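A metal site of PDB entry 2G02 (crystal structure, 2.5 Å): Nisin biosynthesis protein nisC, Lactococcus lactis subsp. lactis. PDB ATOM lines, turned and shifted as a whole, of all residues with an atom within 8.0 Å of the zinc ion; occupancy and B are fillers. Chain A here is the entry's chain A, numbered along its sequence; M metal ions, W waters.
Of the 15 residues printed, 3 come within 4 Å of the zinc ion.
The zinc ion is bound by water W1 (2.0 Å), a ring nitrogen (ND1) of His 325 (2.1 Å), the side-chain sulfur (SG) of Cys 324 (2.3 Å) and the side-chain sulfur (SG) of Cys 278 (2.3 Å). The zinc ion has four donor atoms within binding distance.
A ring nitrogen (NE2) of His 325 sits close to the side-chain sulfur of Met 322, 3.7 Å away. The guanidinium group (NH2) of Arg 274 lies within hydrogen-bond range of the backbone carbonyl oxygen (O) of His 325 (3.5 Å). The backbone carbonyl oxygen of Cys 324 sits at hydrogen-bond distance from the backbone NH of Trp 277, 3.5 Å away. The backbone NH of Cys 324 sits at hydrogen-bond distance from the backbone carbonyl oxygen of Leu 373, at 3.0 Å. The backbone carbonyl oxygen of Cys 278 lies within hydrogen-bond range of the backbone NH of Ala 205, at 3.1 Å.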
ATOM      1  N   ILE A 137     -12.306  11.919  17.673  1.00  0.00           N
ATOM      2  CA  ILE A 137     -12.648  11.816  16.266  1.00  0.00           C
ATOM      3  C   ILE A 137     -11.446  12.105  15.375  1.00  0.00           C
ATOM      4  O   ILE A 137     -11.071  11.251  14.577  1.00  0.00           O
ATOM      5  CB  ILE A 137     -13.918  12.684  15.929  1.00  0.00           C
ATOM      6  CG1 ILE A 137     -15.079  12.336  16.888  1.00  0.00           C
ATOM      7  CG2 ILE A 137     -14.346  12.495  14.473  1.00  0.00           C
ATOM      8  CD1 ILE A 137     -15.377  10.808  16.970  1.00  0.00           C
ATOM      9  N   ALA A 205     -16.623  12.516  22.626  1.00  0.00           N
ATOM     10  CA  ALA A 205     -16.036  12.542  21.293  1.00  0.00           C
ATOM     11  C   ALA A 205     -15.099  13.742  21.052  1.00  0.00           C
ATOM     12  O   ALA A 205     -14.136  13.634  20.307  1.00  0.00           O
ATOM     13  CB  ALA A 205     -17.123  12.487  20.222  1.00  0.00           C
ATOM     14  N   HIS A 206     -15.398  14.879  21.687  1.00  0.00           N
ATOM     15  CA  HIS A 206     -14.734  16.159  21.372  1.00  0.00           C
ATOM     16  C   HIS A 206     -14.168  16.905  22.566  1.00  0.00           C
ATOM     17  O   HIS A 206     -13.559  17.980  22.409  1.00  0.00           O
ATOM     18  CB  HIS A 206     -15.715  17.068  20.626  1.00  0.00           C
ATOM     19  CG  HIS A 206     -16.152  16.538  19.294  1.00  0.00           C
ATOM     20  ND1 HIS A 206     -15.258  16.222  18.302  1.00  0.00           N
ATOM     21  CD2 HIS A 206     -17.388  16.299  18.791  1.00  0.00           C
ATOM     22  CE1 HIS A 206     -15.918  15.797  17.234  1.00  0.00           C
ATOM     23  NE2 HIS A 206     -17.214  15.837  17.505  1.00  0.00           N
ATOM     24  N   ARG A 274     -28.375  15.945  25.261  1.00  0.00           N
ATOM     25  CA  ARG A 274     -28.886  14.663  24.787  1.00  0.00           C
ATOM     26  C   ARG A 274     -28.151  13.476  25.450  1.00  0.00           C
ATOM     27  O   ARG A 274     -27.163  13.682  26.149  1.00  0.00           O
ATOM     28  CB  ARG A 274     -28.793  14.609  23.259  1.00  0.00           C
ATOM     29  CG  ARG A 274     -27.412  14.241  22.727  1.00  0.00           C
ATOM     30  CD  ARG A 274     -27.346  14.312  21.211  1.00  0.00           C
ATOM     31  NE  ARG A 274     -28.347  13.471  20.552  1.00  0.00           N
ATOM     32  CZ  ARG A 274     -28.746  13.651  19.295  1.00  0.00           C
ATOM     33  NH1 ARG A 274     -28.209  14.626  18.572  1.00  0.00           N
ATOM     34  NH2 ARG A 274     -29.654  12.865  18.766  1.00  0.00           N
ATOM     35  N   ALA A 276     -25.985  10.500  24.489  1.00  0.00           N
ATOM     36  CA  ALA A 276     -25.234   9.944  23.389  1.00  0.00           C
ATOM     37  C   ALA A 276     -23.873   9.405  23.813  1.00  0.00           C
ATOM     38  O   ALA A 276     -23.354   9.731  24.890  1.00  0.00           O
ATOM     39  CB  ALA A 276     -25.080  10.982  22.281  1.00  0.00           C
ATOM     40  N   TRP A 277     -23.287   8.580  22.961  1.00  0.00           N
ATOM     41  CA  TRP A 277     -21.884   8.278  23.112  1.00  0.00           C
ATOM     42  C   TRP A 277     -21.054   9.575  23.029  1.00  0.00           C
ATOM     43  O   TRP A 277     -20.218   9.834  23.910  1.00  0.00           O
ATOM     44  CB  TRP A 277     -21.459   7.236  22.052  1.00  0.00           C
ATOM     45  CG  TRP A 277     -19.996   7.001  22.006  1.00  0.00           C
ATOM     46  CD1 TRP A 277     -19.249   6.210  22.838  1.00  0.00           C
ATOM     47  CD2 TRP A 277     -19.091   7.584  21.081  1.00  0.00           C
ATOM     48  NE1 TRP A 277     -17.924   6.261  22.488  1.00  0.00           N
ATOM     49  CE2 TRP A 277     -17.785   7.087  21.404  1.00  0.00           C
ATOM     50  CE3 TRP A 277     -19.234   8.444  19.997  1.00  0.00           C
ATOM     51  CZ2 TRP A 277     -16.646   7.452  20.678  1.00  0.00           C
ATOM     52  CZ3 TRP A 277     -18.094   8.809  19.272  1.00  0.00           C
ATOM     53  CH2 TRP A 277     -16.818   8.317  19.622  1.00  0.00           C
ATOM     54  N   CYS A 278     -21.299  10.388  21.992  1.00  0.00           N
ATOM     55  CA  CYS A 278     -20.437  11.541  21.692  1.00  0.00           C
ATOM     56  C   CYS A 278     -20.545  12.705  22.692  1.00  0.00           C
ATOM     57  O   CYS A 278     -19.537  13.327  23.019  1.00  0.00           O
ATOM     58  CB  CYS A 278     -20.679  12.042  20.253  1.00  0.00           C
ATOM     59  SG  CYS A 278     -22.405  12.456  19.835  1.00  0.00           S
ATOM     60  N   TYR A 279     -21.774  12.994  23.143  1.00  0.00           N
ATOM     61  CA  TYR A 279     -22.039  13.990  24.170  1.00  0.00           C
ATOM     62  C   TYR A 279     -23.037  13.411  25.151  1.00  0.00           C
ATOM     63  O   TYR A 279     -23.995  12.724  24.730  1.00  0.00           O
ATOM     64  CB  TYR A 279     -22.690  15.243  23.579  1.00  0.00           C
ATOM     65  CG  TYR A 279     -21.778  16.145  22.787  1.00  0.00           C
ATOM     66  CD1 TYR A 279     -20.939  17.071  23.412  1.00  0.00           C
ATOM     67  CD2 TYR A 279     -21.815  16.108  21.393  1.00  0.00           C
ATOM     68  CE1 TYR A 279     -20.124  17.953  22.629  1.00  0.00           C
ATOM     69  CE2 TYR A 279     -21.002  16.936  20.622  1.00  0.00           C
ATOM     70  CZ  TYR A 279     -20.167  17.852  21.233  1.00  0.00           C
ATOM     71  OH  TYR A 279     -19.397  18.654  20.422  1.00  0.00           O
ATOM     72  N   MET A 322     -28.419   4.710  15.257  1.00  0.00           N
ATOM     73  CA  MET A 322     -27.020   4.882  14.912  1.00  0.00           C
ATOM     74  C   MET A 322     -26.122   4.796  16.158  1.00  0.00           C
ATOM     75  O   MET A 322     -26.604   4.916  17.295  1.00  0.00           O
ATOM     76  CB  MET A 322     -26.833   6.227  14.229  1.00  0.00           C
ATOM     77  CG  MET A 322     -26.600   7.348  15.199  1.00  0.00           C
ATOM     78  SD  MET A 322     -26.269   8.854  14.332  1.00  0.00           S
ATOM     79  CE  MET A 322     -24.818   9.347  15.133  1.00  0.00           C
ATOM     80  N   ILE A 323     -24.814   4.620  15.925  1.00  0.00           N
ATOM     81  CA  ILE A 323     -23.849   4.567  16.998  1.00  0.00           C
ATOM     82  C   ILE A 323     -23.560   5.935  17.644  1.00  0.00           C
ATOM     83  O   ILE A 323     -23.597   6.073  18.875  1.00  0.00           O
ATOM     84  CB  ILE A 323     -22.520   3.892  16.489  1.00  0.00           C
ATOM     85  CG1 ILE A 323     -22.706   2.377  16.434  1.00  0.00           C
ATOM     86  CG2 ILE A 323     -21.288   4.273  17.364  1.00  0.00           C
ATOM     87  CD1 ILE A 323     -21.473   1.640  16.101  1.00  0.00           C
ATOM     88  N   CYS A 324     -23.258   6.938  16.836  1.00  0.00           N
ATOM     89  CA  CYS A 324     -22.643   8.163  17.363  1.00  0.00           C
ATOM     90  C   CYS A 324     -23.496   8.866  18.425  1.00  0.00           C
ATOM     91  O   CYS A 324     -23.047   9.096  19.545  1.00  0.00           O
ATOM     92  CB  CYS A 324     -22.261   9.135  16.223  1.00  0.00           C
ATOM     93  SG  CYS A 324     -21.267  10.579  16.737  1.00  0.00           S
ATOM     94  N   HIS A 325     -24.734   9.173  18.073  1.00  0.00           N
ATOM     95  CA  HIS A 325     -25.665   9.801  18.986  1.00  0.00           C
ATOM     96  C   HIS A 325     -27.036   9.133  18.843  1.00  0.00           C
ATOM     97  O   HIS A 325     -28.063   9.796  18.924  1.00  0.00           O
ATOM     98  CB  HIS A 325     -25.718  11.343  18.779  1.00  0.00           C
ATOM     99  CG  HIS A 325     -25.670  11.795  17.341  1.00  0.00           C
ATOM    100  ND1 HIS A 325     -24.495  12.105  16.690  1.00  0.00           N
ATOM    101  CD2 HIS A 325     -26.675  12.004  16.441  1.00  0.00           C
ATOM    102  CE1 HIS A 325     -24.771  12.494  15.451  1.00  0.00           C
ATOM    103  NE2 HIS A 325     -26.085  12.440  15.276  1.00  0.00           N
ATOM    104  N   GLY A 326     -27.027   7.821  18.600  1.00  0.00           N
ATOM    105  CA  GLY A 326     -28.253   7.005  18.580  1.00  0.00           C
ATOM    106  C   GLY A 326     -28.272   5.850  19.596  1.00  0.00           C
ATOM    107  O   GLY A 326     -27.354   5.699  20.414  1.00  0.00           O
ATOM    108  N   LEU A 373     -20.029   5.118  11.765  1.00  0.00           N
ATOM    109  CA  LEU A 373     -20.348   6.022  12.849  1.00  0.00           C
ATOM    110  C   LEU A 373     -21.821   6.416  12.862  1.00  0.00           C
ATOM    111  O   LEU A 373     -22.453   6.546  13.929  1.00  0.00           O
ATOM    112  CB  LEU A 373     -19.407   7.226  12.815  1.00  0.00           C
ATOM    113  CG  LEU A 373     -19.366   8.199  13.990  1.00  0.00           C
ATOM    114  CD1 LEU A 373     -19.080   7.490  15.316  1.00  0.00           C
ATOM    115  CD2 LEU A 373     -18.408   9.378  13.751  1.00  0.00           C
ATOM    116  N   GLU A 374     -22.392   6.584  11.685  1.00  0.00           N
ATOM    117  CA  GLU A 374     -23.790   6.969  11.627  1.00  0.00           C
ATOM    118  C   GLU A 374     -24.624   6.025  10.812  1.00  0.00           C
ATOM    119  O   GLU A 374     -25.853   6.063  10.899  1.00  0.00           O
ATOM    120  CB  GLU A 374     -23.951   8.379  11.070  1.00  0.00           C
ATOM    121  CG  GLU A 374     -23.309   9.399  11.973  1.00  0.00           C
ATOM    122  CD  GLU A 374     -23.612  10.799  11.553  1.00  0.00           C
ATOM    123  OE1 GLU A 374     -24.146  10.966  10.439  1.00  0.00           O
ATOM    124  OE2 GLU A 374     -23.302  11.723  12.317  1.00  0.00           O
HETATM  125 ZN    ZN M   1     -22.632  12.153  17.590  1.00  0.00          ZN
HETATM  126  O   HOH W   1     -21.717  13.790  16.843  1.00  0.00           O
